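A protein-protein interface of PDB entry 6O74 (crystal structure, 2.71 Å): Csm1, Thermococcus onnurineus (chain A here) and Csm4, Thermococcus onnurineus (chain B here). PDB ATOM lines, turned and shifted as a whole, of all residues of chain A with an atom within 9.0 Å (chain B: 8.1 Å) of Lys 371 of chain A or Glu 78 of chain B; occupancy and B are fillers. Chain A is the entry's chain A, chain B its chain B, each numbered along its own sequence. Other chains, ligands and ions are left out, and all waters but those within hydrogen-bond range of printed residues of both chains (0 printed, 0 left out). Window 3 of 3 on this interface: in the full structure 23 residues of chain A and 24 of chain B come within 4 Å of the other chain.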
ATOM      1  N   LEU A 249      -5.055 -17.158   8.672  1.00  0.00           N
ATOM      2  CA  LEU A 249      -5.811 -15.969   9.158  1.00  0.00           C
ATOM      3  C   LEU A 249      -4.825 -15.038   9.868  1.00  0.00           C
ATOM      4  O   LEU A 249      -4.290 -15.446  10.910  1.00  0.00           O
ATOM      5  CB  LEU A 249      -6.922 -16.382  10.129  1.00  0.00           C
ATOM      6  CG  LEU A 249      -8.128 -17.094   9.526  1.00  0.00           C
ATOM      7  CD1 LEU A 249      -9.182 -17.336  10.592  1.00  0.00           C
ATOM      8  CD2 LEU A 249      -8.723 -16.304   8.370  1.00  0.00           C
ATOM      9  N   GLU A 251      -4.605 -11.501  11.772  1.00  0.00           N
ATOM     10  CA  GLU A 251      -5.350 -10.397  12.435  1.00  0.00           C
ATOM     11  C   GLU A 251      -4.341  -9.365  12.964  1.00  0.00           C
ATOM     12  O   GLU A 251      -3.419  -9.740  13.692  1.00  0.00           O
ATOM     13  CB  GLU A 251      -6.283 -10.961  13.511  1.00  0.00           C
ATOM     14  CG  GLU A 251      -7.611 -10.220  13.611  1.00  0.00           C
ATOM     15  CD  GLU A 251      -8.699 -10.893  14.436  1.00  0.00           C
ATOM     16  OE1 GLU A 251      -9.154 -11.993  14.038  1.00  0.00           O
ATOM     17  OE2 GLU A 251      -9.102 -10.311  15.475  1.00  0.00           O
ATOM     18  N   MET A 311      -7.889  -7.861   9.021  1.00  0.00           N
ATOM     19  CA  MET A 311      -7.843  -9.339   8.870  1.00  0.00           C
ATOM     20  C   MET A 311      -7.497  -9.659   7.412  1.00  0.00           C
ATOM     21  O   MET A 311      -8.089  -9.020   6.508  1.00  0.00           O
ATOM     22  CB  MET A 311      -9.177 -10.000   9.227  1.00  0.00           C
ATOM     23  CG  MET A 311      -9.174 -11.503   8.989  1.00  0.00           C
ATOM     24  SD  MET A 311     -10.716 -12.326   9.464  1.00  0.00           S
ATOM     25  CE  MET A 311     -10.400 -12.609  11.205  1.00  0.00           C
ATOM     26  N   GLU A 350      -2.445 -17.540  12.216  1.00  0.00           N
ATOM     27  CA  GLU A 350      -2.793 -18.916  12.638  1.00  0.00           C
ATOM     28  C   GLU A 350      -2.861 -19.826  11.418  1.00  0.00           C
ATOM     29  O   GLU A 350      -3.535 -19.502  10.438  1.00  0.00           O
ATOM     30  CB  GLU A 350      -4.128 -18.895  13.377  1.00  0.00           C
ATOM     31  CG  GLU A 350      -4.377 -20.149  14.184  1.00  0.00           C
ATOM     32  CD  GLU A 350      -5.707 -20.139  14.907  1.00  0.00           C
ATOM     33  OE1 GLU A 350      -5.850 -20.922  15.870  1.00  0.00           O
ATOM     34  OE2 GLU A 350      -6.592 -19.347  14.503  1.00  0.00           O
ATOM     35  N   ASN A 364     -19.457 -25.034  13.960  1.00  0.00           N
ATOM     36  CA  ASN A 364     -18.956 -23.747  13.398  1.00  0.00           C
ATOM     37  C   ASN A 364     -17.471 -23.602  13.728  1.00  0.00           C
ATOM     38  O   ASN A 364     -17.162 -23.195  14.857  1.00  0.00           O
ATOM     39  CB  ASN A 364     -19.711 -22.521  13.923  1.00  0.00           C
ATOM     40  CG  ASN A 364     -19.249 -21.238  13.262  1.00  0.00           C
ATOM     41  OD1 ASN A 364     -18.230 -21.221  12.570  1.00  0.00           O
ATOM     42  ND2 ASN A 364     -19.997 -20.160  13.445  1.00  0.00           N
ATOM     43  N   LEU A 365     -16.603 -23.889  12.757  1.00  0.00           N
ATOM     44  CA  LEU A 365     -15.128 -23.955  12.936  1.00  0.00           C
ATOM     45  C   LEU A 365     -14.481 -22.595  12.640  1.00  0.00           C
ATOM     46  O   LEU A 365     -13.432 -22.311  13.253  1.00  0.00           O
ATOM     47  CB  LEU A 365     -14.567 -25.042  12.015  1.00  0.00           C
ATOM     48  CG  LEU A 365     -15.124 -26.448  12.229  1.00  0.00           C
ATOM     49  CD1 LEU A 365     -14.464 -27.418  11.264  1.00  0.00           C
ATOM     50  CD2 LEU A 365     -14.937 -26.912  13.670  1.00  0.00           C
ATOM     51  N   PHE A 366     -15.054 -21.802  11.726  1.00  0.00           N
ATOM     52  CA  PHE A 366     -14.534 -20.459  11.353  1.00  0.00           C
ATOM     53  C   PHE A 366     -14.524 -19.560  12.592  1.00  0.00           C
ATOM     54  O   PHE A 366     -13.467 -19.002  12.919  1.00  0.00           O
ATOM     55  CB  PHE A 366     -15.356 -19.831  10.227  1.00  0.00           C
ATOM     56  CG  PHE A 366     -14.767 -18.564   9.664  1.00  0.00           C
ATOM     57  CD1 PHE A 366     -13.435 -18.506   9.277  1.00  0.00           C
ATOM     58  CD2 PHE A 366     -15.551 -17.433   9.484  1.00  0.00           C
ATOM     59  CE1 PHE A 366     -12.897 -17.347   8.736  1.00  0.00           C
ATOM     60  CE2 PHE A 366     -15.012 -16.272   8.944  1.00  0.00           C
ATOM     61  CZ  PHE A 366     -13.688 -16.232   8.568  1.00  0.00           C
ATOM     62  N   ALA A 367     -15.673 -19.445  13.257  1.00  0.00           N
ATOM     63  CA  ALA A 367     -15.829 -18.757  14.558  1.00  0.00           C
ATOM     64  C   ALA A 367     -14.778 -19.294  15.540  1.00  0.00           C
ATOM     65  O   ALA A 367     -14.053 -18.471  16.139  1.00  0.00           O
ATOM     66  CB  ALA A 367     -17.234 -18.958  15.073  1.00  0.00           C
ATOM     67  N   GLU A 368     -14.704 -20.622  15.674  1.00  0.00           N
ATOM     68  CA  GLU A 368     -13.770 -21.352  16.576  1.00  0.00           C
ATOM     69  C   GLU A 368     -12.329 -20.925  16.257  1.00  0.00           C
ATOM     70  O   GLU A 368     -11.506 -20.871  17.189  1.00  0.00           O
ATOM     71  CB  GLU A 368     -13.929 -22.871  16.414  1.00  0.00           C
ATOM     72  CG  GLU A 368     -14.021 -23.643  17.725  1.00  0.00           C
ATOM     73  CD  GLU A 368     -12.825 -23.516  18.662  1.00  0.00           C
ATOM     74  OE1 GLU A 368     -12.961 -22.832  19.700  1.00  0.00           O
ATOM     75  OE2 GLU A 368     -11.760 -24.107  18.365  1.00  0.00           O
ATOM     76  N   ALA A 369     -12.031 -20.660  14.983  1.00  0.00           N
ATOM     77  CA  ALA A 369     -10.673 -20.352  14.478  1.00  0.00           C
ATOM     78  C   ALA A 369     -10.352 -18.884  14.755  1.00  0.00           C
ATOM     79  O   ALA A 369      -9.209 -18.585  15.155  1.00  0.00           O
ATOM     80  CB  ALA A 369     -10.587 -20.659  13.004  1.00  0.00           C
ATOM     81  N   ARG A 370     -11.335 -18.014  14.526  1.00  0.00           N
ATOM     82  CA  ARG A 370     -11.282 -16.571  14.871  1.00  0.00           C
ATOM     83  C   ARG A 370     -11.118 -16.432  16.393  1.00  0.00           C
ATOM     84  O   ARG A 370     -10.285 -15.614  16.812  1.00  0.00           O
ATOM     85  CB  ARG A 370     -12.505 -15.850  14.287  1.00  0.00           C
ATOM     86  CG  ARG A 370     -12.349 -15.510  12.809  1.00  0.00           C
ATOM     87  CD  ARG A 370     -13.560 -14.878  12.145  1.00  0.00           C
ATOM     88  NE  ARG A 370     -14.512 -14.270  13.072  1.00  0.00           N
ATOM     89  CZ  ARG A 370     -14.413 -13.051  13.605  1.00  0.00           C
ATOM     90  NH1 ARG A 370     -13.384 -12.263  13.326  1.00  0.00           N
ATOM     91  NH2 ARG A 370     -15.356 -12.623  14.428  1.00  0.00           N
ATOM     92  N   LYS A 371     -11.833 -17.228  17.189  1.00  0.00           N
ATOM     93  CA  LYS A 371     -11.750 -17.190  18.677  1.00  0.00           C
ATOM     94  C   LYS A 371     -10.315 -17.516  19.123  1.00  0.00           C
ATOM     95  O   LYS A 371      -9.754 -16.730  19.908  1.00  0.00           O
ATOM     96  CB  LYS A 371     -12.771 -18.140  19.311  1.00  0.00           C
ATOM     97  CG  LYS A 371     -13.158 -17.799  20.742  1.00  0.00           C
ATOM     98  CD  LYS A 371     -14.504 -18.348  21.177  1.00  0.00           C
ATOM     99  CE  LYS A 371     -15.155 -17.504  22.255  1.00  0.00           C
ATOM    100  NZ  LYS A 371     -16.345 -18.167  22.838  1.00  0.00           N
ATOM    101  N   ARG A 372      -9.737 -18.620  18.638  1.00  0.00           N
ATOM    102  CA  ARG A 372      -8.330 -19.028  18.922  1.00  0.00           C
ATOM    103  C   ARG A 372      -7.366 -17.898  18.528  1.00  0.00           C
ATOM    104  O   ARG A 372      -6.331 -17.736  19.215  1.00  0.00           O
ATOM    105  CB  ARG A 372      -7.947 -20.320  18.185  1.00  0.00           C
ATOM    106  CG  ARG A 372      -8.330 -21.607  18.909  1.00  0.00           C
ATOM    107  CD  ARG A 372      -7.593 -22.845  18.408  1.00  0.00           C
ATOM    108  NE  ARG A 372      -7.508 -22.921  16.952  1.00  0.00           N
ATOM    109  CZ  ARG A 372      -8.523 -23.221  16.142  1.00  0.00           C
ATOM    110  NH1 ARG A 372      -9.726 -23.479  16.632  1.00  0.00           N
ATOM    111  NH2 ARG A 372      -8.337 -23.243  14.834  1.00  0.00           N
ATOM    112  N   LEU A 373      -7.672 -17.151  17.463  1.00  0.00           N
ATOM    113  CA  LEU A 373      -6.787 -16.070  16.953  1.00  0.00           C
ATOM    114  C   LEU A 373      -6.939 -14.808  17.820  1.00  0.00           C
ATOM    115  O   LEU A 373      -5.899 -14.191  18.128  1.00  0.00           O
ATOM    116  CB  LEU A 373      -7.117 -15.799  15.484  1.00  0.00           C
ATOM    117  CG  LEU A 373      -6.311 -14.691  14.813  1.00  0.00           C
ATOM    118  CD1 LEU A 373      -4.815 -14.912  14.976  1.00  0.00           C
ATOM    119  CD2 LEU A 373      -6.668 -14.602  13.343  1.00  0.00           C
ATOM    120  N   LYS A 374      -8.172 -14.434  18.191  1.00  0.00           N
ATOM    121  CA  LYS A 374      -8.460 -13.324  19.146  1.00  0.00           C
ATOM    122  C   LYS A 374      -7.635 -13.557  20.422  1.00  0.00           C
ATOM    123  O   LYS A 374      -6.972 -12.604  20.880  1.00  0.00           O
ATOM    124  CB  LYS A 374      -9.965 -13.218  19.435  1.00  0.00           C
ATOM    125  CG  LYS A 374     -10.380 -12.149  20.444  1.00  0.00           C
ATOM    126  CD  LYS A 374     -10.113 -10.711  19.989  1.00  0.00           C
ATOM    127  CE  LYS A 374      -9.804  -9.735  21.116  1.00  0.00           C
ATOM    128  NZ  LYS A 374      -8.380  -9.309  21.137  1.00  0.00           N
ATOM    129  N   HIS A 375      -7.637 -14.784  20.954  1.00  0.00           N
ATOM    130  CA  HIS A 375      -6.848 -15.174  22.154  1.00  0.00           C
ATOM    131  C   HIS A 375      -5.374 -14.812  21.943  1.00  0.00           C
ATOM    132  O   HIS A 375      -4.782 -14.185  22.831  1.00  0.00           O
ATOM    133  CB  HIS A 375      -7.019 -16.659  22.485  1.00  0.00           C
ATOM    134  CG  HIS A 375      -6.378 -17.035  23.778  1.00  0.00           C
ATOM    135  ND1 HIS A 375      -5.128 -17.624  23.838  1.00  0.00           N
ATOM    136  CD2 HIS A 375      -6.789 -16.877  25.056  1.00  0.00           C
ATOM    137  CE1 HIS A 375      -4.803 -17.831  25.099  1.00  0.00           C
ATOM    138  NE2 HIS A 375      -5.806 -17.380  25.868  1.00  0.00           N
ATOM    139  N   LYS A 376      -4.797 -15.186  20.805  1.00  0.00           N
ATOM    140  CA  LYS A 376      -3.379 -14.877  20.502  1.00  0.00           C
ATOM    141  C   LYS A 376      -3.175 -13.357  20.587  1.00  0.00           C
ATOM    142  O   LYS A 376      -2.120 -12.938  21.093  1.00  0.00           O
ATOM    143  CB  LYS A 376      -2.979 -15.422  19.128  1.00  0.00           C
ATOM    144  CG  LYS A 376      -2.770 -16.930  19.040  1.00  0.00           C
ATOM    145  CD  LYS A 376      -1.818 -17.312  17.916  1.00  0.00           C
ATOM    146  CE  LYS A 376      -2.162 -18.612  17.220  1.00  0.00           C
ATOM    147  NZ  LYS A 376      -1.108 -19.637  17.403  1.00  0.00           N
ATOM    148  N   LEU A 377      -4.149 -12.566  20.116  1.00  0.00           N
ATOM    149  CA  LEU A 377      -4.058 -11.079  20.058  1.00  0.00           C
ATOM    150  C   LEU A 377      -4.121 -10.501  21.472  1.00  0.00           C
ATOM    151  O   LEU A 377      -3.397  -9.524  21.736  1.00  0.00           O
ATOM    152  CB  LEU A 377      -5.192 -10.505  19.206  1.00  0.00           C
ATOM    153  CG  LEU A 377      -4.891 -10.269  17.730  1.00  0.00           C
ATOM    154  CD1 LEU A 377      -6.060  -9.546  17.078  1.00  0.00           C
ATOM    155  CD2 LEU A 377      -3.614  -9.469  17.532  1.00  0.00           C
ATOM    156  N   THR A 378      -4.978 -11.054  22.332  1.00  0.00           N
ATOM    157  CA  THR A 378      -5.091 -10.632  23.751  1.00  0.00           C
ATOM    158  C   THR A 378      -3.730 -10.851  24.424  1.00  0.00           C
ATOM    159  O   THR A 378      -3.241  -9.897  25.051  1.00  0.00           O
ATOM    160  CB  THR A 378      -6.263 -11.321  24.458  1.00  0.00           C
ATOM    161  OG1 THR A 378      -6.455 -12.592  23.845  1.00  0.00           O
ATOM    162  CG2 THR A 378      -7.552 -10.533  24.372  1.00  0.00           C
ATOM    163  N   GLY A 540     -19.026  -7.992  18.514  1.00  0.00           N
ATOM    164  CA  GLY A 540     -18.152  -9.181  18.557  1.00  0.00           C
ATOM    165  C   GLY A 540     -18.969 -10.461  18.598  1.00  0.00           C
ATOM    166  O   GLY A 540     -18.585 -11.437  17.925  1.00  0.00           O
ATOM    167  N   GLU A 541     -20.064 -10.438  19.361  1.00  0.00           N
ATOM    168  CA  GLU A 541     -21.024 -11.556  19.531  1.00  0.00           C
ATOM    169  C   GLU A 541     -21.683 -11.831  18.178  1.00  0.00           C
ATOM    170  O   GLU A 541     -21.713 -13.001  17.754  1.00  0.00           O
ATOM    171  CB  GLU A 541     -22.039 -11.183  20.614  1.00  0.00           C
ATOM    172  CG  GLU A 541     -22.999 -12.298  20.983  1.00  0.00           C
ATOM    173  CD  GLU A 541     -23.638 -12.175  22.359  1.00  0.00           C
ATOM    174  OE1 GLU A 541     -23.018 -11.555  23.265  1.00  0.00           O
ATOM    175  OE2 GLU A 541     -24.758 -12.706  22.526  1.00  0.00           O
ATOM    176  N   PHE A 543     -20.733 -10.899  15.072  1.00  0.00           N
ATOM    177  CA  PHE A 543     -19.700 -11.334  14.093  1.00  0.00           C
ATOM    178  C   PHE A 543     -19.305 -12.793  14.338  1.00  0.00           C
ATOM    179  O   PHE A 543     -18.988 -13.499  13.357  1.00  0.00           O
ATOM    180  CB  PHE A 543     -18.439 -10.468  14.174  1.00  0.00           C
ATOM    181  CG  PHE A 543     -18.498  -9.144  13.461  1.00  0.00           C
ATOM    182  CD1 PHE A 543     -19.425  -8.896  12.457  1.00  0.00           C
ATOM    183  CD2 PHE A 543     -17.601  -8.148  13.787  1.00  0.00           C
ATOM    184  CE1 PHE A 543     -19.459  -7.673  11.808  1.00  0.00           C
ATOM    185  CE2 PHE A 543     -17.632  -6.930  13.133  1.00  0.00           C
ATOM    186  CZ  PHE A 543     -18.561  -6.694  12.146  1.00  0.00           C
ATOM    187  N   SER A 544     -19.285 -13.208  15.607  1.00  0.00           N
ATOM    188  CA  SER A 544     -18.969 -14.590  16.048  1.00  0.00           C
ATOM    189  C   SER A 544     -19.977 -15.579  15.446  1.00  0.00           C
ATOM    190  O   SER A 544     -19.597 -16.746  15.235  1.00  0.00           O
ATOM    191  CB  SER A 544     -18.937 -14.674  17.549  1.00  0.00           C
ATOM    192  OG  SER A 544     -18.701 -16.007  17.966  1.00  0.00           O
ATOM    193  N   VAL B  73      -4.774 -13.686  34.663  1.00  0.00           N
ATOM    194  CA  VAL B  73      -6.187 -14.154  34.500  1.00  0.00           C
ATOM    195  C   VAL B  73      -6.818 -13.569  33.231  1.00  0.00           C
ATOM    196  O   VAL B  73      -7.836 -14.127  32.802  1.00  0.00           O
ATOM    197  CB  VAL B  73      -7.054 -13.823  35.729  1.00  0.00           C
ATOM    198  CG1 VAL B  73      -6.417 -14.314  37.019  1.00  0.00           C
ATOM    199  CG2 VAL B  73      -7.384 -12.341  35.821  1.00  0.00           C
ATOM    200  N   GLU B  74      -6.261 -12.494  32.667  1.00  0.00           N
ATOM    201  CA  GLU B  74      -6.809 -11.826  31.453  1.00  0.00           C
ATOM    202  C   GLU B  74      -7.009 -12.865  30.347  1.00  0.00           C
ATOM    203  O   GLU B  74      -8.078 -12.928  29.745  1.00  0.00           O
ATOM    204  CB  GLU B  74      -5.898 -10.701  30.947  1.00  0.00           C
ATOM    205  CG  GLU B  74      -5.541  -9.640  31.975  1.00  0.00           C
ATOM    206  CD  GLU B  74      -6.568  -8.536  32.121  1.00  0.00           C
ATOM    207  OE1 GLU B  74      -7.759  -8.868  32.247  1.00  0.00           O
ATOM    208  OE2 GLU B  74      -6.171  -7.354  32.089  1.00  0.00           O
ATOM    209  N   PRO B  75      -6.004 -13.715  30.035  1.00  0.00           N
ATOM    210  CA  PRO B  75      -6.148 -14.733  28.995  1.00  0.00           C
ATOM    211  C   PRO B  75      -6.838 -16.031  29.450  1.00  0.00           C
ATOM    212  O   PRO B  75      -6.961 -16.924  28.643  1.00  0.00           O
ATOM    213  CB  PRO B  75      -4.693 -15.064  28.605  1.00  0.00           C
ATOM    214  CG  PRO B  75      -3.818 -14.141  29.439  1.00  0.00           C
ATOM    215  CD  PRO B  75      -4.661 -13.751  30.631  1.00  0.00           C
ATOM    216  N   ALA B  76      -7.245 -16.121  30.719  1.00  0.00           N
ATOM    217  CA  ALA B  76      -7.853 -17.326  31.332  1.00  0.00           C
ATOM    218  C   ALA B  76      -9.367 -17.146  31.509  1.00  0.00           C
ATOM    219  O   ALA B  76     -10.021 -18.131  31.903  1.00  0.00           O
ATOM    220  CB  ALA B  76      -7.195 -17.606  32.662  1.00  0.00           C
ATOM    221  N   LEU B  77      -9.902 -15.950  31.229  1.00  0.00           N
ATOM    222  CA  LEU B  77     -11.239 -15.509  31.716  1.00  0.00           C
ATOM    223  C   LEU B  77     -12.324 -16.500  31.272  1.00  0.00           C
ATOM    224  O   LEU B  77     -13.376 -16.544  31.942  1.00  0.00           O
ATOM    225  CB  LEU B  77     -11.526 -14.082  31.238  1.00  0.00           C
ATOM    226  CG  LEU B  77     -10.745 -12.985  31.966  1.00  0.00           C
ATOM    227  CD1 LEU B  77     -10.861 -11.652  31.243  1.00  0.00           C
ATOM    228  CD2 LEU B  77     -11.198 -12.838  33.415  1.00  0.00           C
ATOM    229  N   GLU B  78     -12.072 -17.278  30.213  1.00  0.00           N
ATOM    230  CA  GLU B  78     -12.888 -18.469  29.845  1.00  0.00           C
ATOM    231  C   GLU B  78     -12.351 -19.687  30.615  1.00  0.00           C
ATOM    232  O   GLU B  78     -11.766 -20.591  29.982  1.00  0.00           O
ATOM    233  CB  GLU B  78     -12.898 -18.651  28.326  1.00  0.00           C
ATOM    234  CG  GLU B  78     -13.426 -17.431  27.585  1.00  0.00           C
ATOM    235  CD  GLU B  78     -14.402 -17.704  26.450  1.00  0.00           C
ATOM    236  OE1 GLU B  78     -14.990 -18.808  26.417  1.00  0.00           O
ATOM    237  OE2 GLU B  78     -14.587 -16.804  25.606  1.00  0.00           O
ATOM    238  N   GLY B  79     -12.542 -19.686  31.940  1.00  0.00           N
ATOM    239  CA  GLY B  79     -12.098 -20.741  32.870  1.00  0.00           C
ATOM    240  C   GLY B  79     -12.858 -20.677  34.186  1.00  0.00           C
ATOM    241  O   GLY B  79     -13.731 -19.785  34.303  1.00  0.00           O
ATOM    242  N   GLU B  86     -24.233 -16.866  27.711  1.00  0.00           N
ATOM    243  CA  GLU B  86     -23.299 -16.215  26.740  1.00  0.00           C
ATOM    244  C   GLU B  86     -23.376 -14.681  26.864  1.00  0.00           C
ATOM    245  O   GLU B  86     -22.358 -14.018  26.558  1.00  0.00           O
ATOM    246  CB  GLU B  86     -23.615 -16.677  25.310  1.00  0.00           C
ATOM    247  CG  GLU B  86     -22.678 -16.121  24.241  1.00  0.00           C
ATOM    248  CD  GLU B  86     -23.188 -16.195  22.807  1.00  0.00           C
ATOM    249  OE1 GLU B  86     -24.346 -16.614  22.601  1.00  0.00           O
ATOM    250  OE2 GLU B  86     -22.421 -15.827  21.896  1.00  0.00           O
ATOM    251  N   ARG B  89     -21.493 -14.017  30.066  1.00  0.00           N
ATOM    252  CA  ARG B  89     -20.055 -14.322  29.817  1.00  0.00           C
ATOM    253  C   ARG B  89     -19.353 -13.074  29.263  1.00  0.00           C
ATOM    254  O   ARG B  89     -18.335 -12.680  29.855  1.00  0.00           O
ATOM    255  CB  ARG B  89     -19.902 -15.537  28.889  1.00  0.00           C
ATOM    256  CG  ARG B  89     -20.131 -16.879  29.576  1.00  0.00           C
ATOM    257  CD  ARG B  89     -20.470 -18.025  28.634  1.00  0.00           C
ATOM    258  NE  ARG B  89     -21.391 -18.994  29.229  1.00  0.00           N
ATOM    259  CZ  ARG B  89     -21.092 -20.241  29.606  1.00  0.00           C
ATOM    260  NH1 ARG B  89     -19.870 -20.726  29.457  1.00  0.00           N
ATOM    261  NH2 ARG B  89     -22.032 -21.011  30.130  1.00  0.00           N
ATOM    262  N   TYR B  90     -19.885 -12.463  28.198  1.00  0.00           N
ATOM    263  CA  TYR B  90     -19.283 -11.287  27.504  1.00  0.00           C
ATOM    264  C   TYR B  90     -19.297 -10.056  28.421  1.00  0.00           C
ATOM    265  O   TYR B  90     -18.255  -9.376  28.500  1.00  0.00           O
ATOM    266  CB  TYR B  90     -19.984 -10.991  26.172  1.00  0.00           C
ATOM    267  CG  TYR B  90     -19.236 -11.463  24.948  1.00  0.00           C
ATOM    268  CD1 TYR B  90     -18.344 -10.629  24.289  1.00  0.00           C
ATOM    269  CD2 TYR B  90     -19.415 -12.743  24.443  1.00  0.00           C
ATOM    270  CE1 TYR B  90     -17.652 -11.052  23.164  1.00  0.00           C
ATOM    271  CE2 TYR B  90     -18.730 -13.183  23.320  1.00  0.00           C
ATOM    272  CZ  TYR B  90     -17.846 -12.334  22.678  1.00  0.00           C
ATOM    273  OH  TYR B  90     -17.168 -12.757  21.572  1.00  0.00           O
ATOM    274  N   ALA B  93     -17.046 -10.587  31.839  1.00  0.00           N
ATOM    275  CA  ALA B  93     -15.633 -10.758  31.418  1.00  0.00           C
ATOM    276  C   ALA B  93     -15.010  -9.403  31.057  1.00  0.00           C
ATOM    277  O   ALA B  93     -13.799  -9.244  31.291  1.00  0.00           O
ATOM    278  CB  ALA B  93     -15.529 -11.720  30.258  1.00  0.00           C
ATOM    279  N   ARG B  97     -11.917  -7.354  33.148  1.00  0.00           N
ATOM    280  CA  ARG B  97     -10.782  -6.874  32.316  1.00  0.00           C
ATOM    281  C   ARG B  97     -10.508  -5.389  32.602  1.00  0.00           C
ATOM    282  O   ARG B  97      -9.417  -4.925  32.232  1.00  0.00           O
ATOM    283  CB  ARG B  97     -11.077  -7.128  30.831  1.00  0.00           C
ATOM    284  CG  ARG B  97      -9.837  -7.296  29.963  1.00  0.00           C
ATOM    285  CD  ARG B  97     -10.165  -7.449  28.488  1.00  0.00           C
ATOM    286  NE  ARG B  97     -10.509  -8.820  28.122  1.00  0.00           N
ATOM    287  CZ  ARG B  97      -9.647  -9.756  27.718  1.00  0.00           C
ATOM    288  NH1 ARG B  97     -10.087 -10.965  27.406  1.00  0.00           N
ATOM    289  NH2 ARG B  97      -8.354  -9.493  27.627  1.00  0.00           N
ATOM    290  N   PRO B 285      -2.215 -20.339  32.997  1.00  0.00           N
ATOM    291  CA  PRO B 285      -2.818 -21.254  32.032  1.00  0.00           C
ATOM    292  C   PRO B 285      -1.865 -21.452  30.843  1.00  0.00           C
ATOM    293  O   PRO B 285      -1.130 -20.530  30.531  1.00  0.00           O
ATOM    294  CB  PRO B 285      -4.103 -20.514  31.648  1.00  0.00           C
ATOM    295  CG  PRO B 285      -3.704 -19.054  31.711  1.00  0.00           C
ATOM    296  CD  PRO B 285      -2.742 -18.969  32.875  1.00  0.00           C
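NE2 of His 375 of chain A lies within hydrogen-bond range of O of Pro 75 of chain B (3.0 Å). The side-chain carboxylate (OE2) of Glu 78 of chain B lies within salt-bridge range of the side-chain amino group (NZ) of Lys 371 of chain A (3.6 Å).
O of Lys 374 of chain A lies within hydrogen-bond range of OG1 of Thr 378 of chain A. O of His 375 of chain A lies within hydrogen-bond range of OG1 of Thr 378 of chain A (2.5 Å).
Among the printed residues, pairs that only touch across the chains: Thr 378 of chain A with Arg 97 of chain B (3.5 Å), Glu 541 of chain A with Glu 86 of chain B (3.7 Å) and Glu 541 of chain A with Tyr 90 of chain B (3.97 Å).
Of the printed residues of chain B, Thr 378 of chain A touches Arg 97. Of the printed residues of chain B, Glu 541 of chain A touches Glu 86 (3.7 Å) and Tyr 90 (3.97 Å). Glu 78 of chain B touches one residue of chain A. Gly 79 of chain B touches none of the printed residues of chain A. Printed residues of chain A within 4 Å of Glu 86 of chain B: Glu 541 (3.7 Å). Of the printed residues of chain A, Tyr 90 of chain B touches Glu 541 (3.97 Å). Of the printed residues of chain A, Arg 97 of chain B touches Thr 378. The nearest residue of chain A that does not touch Glu 78 of chain B is His 375 of chain A (7.1 Å). The nearest printed residue of chain B that does not touch Thr 378 of chain A is Pro 75 of chain B (5.6 Å).
Hydrophobic or aromatic side chains of chain B that line the printed part of chain A: Pro 75 and Tyr 90. Hydrophobic or aromatic side chains of chain A that line the printed part of chain B: His 375. Along chain A the printed residues that touch a printed residue of chain B span positions 371 to 541. Among the printed residues, Asp or Glu carboxylates within 4 Å of a Lys or Arg side-chain nitrogen of the other chain: Lys 371 of chain A with Glu 78 of chain B.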
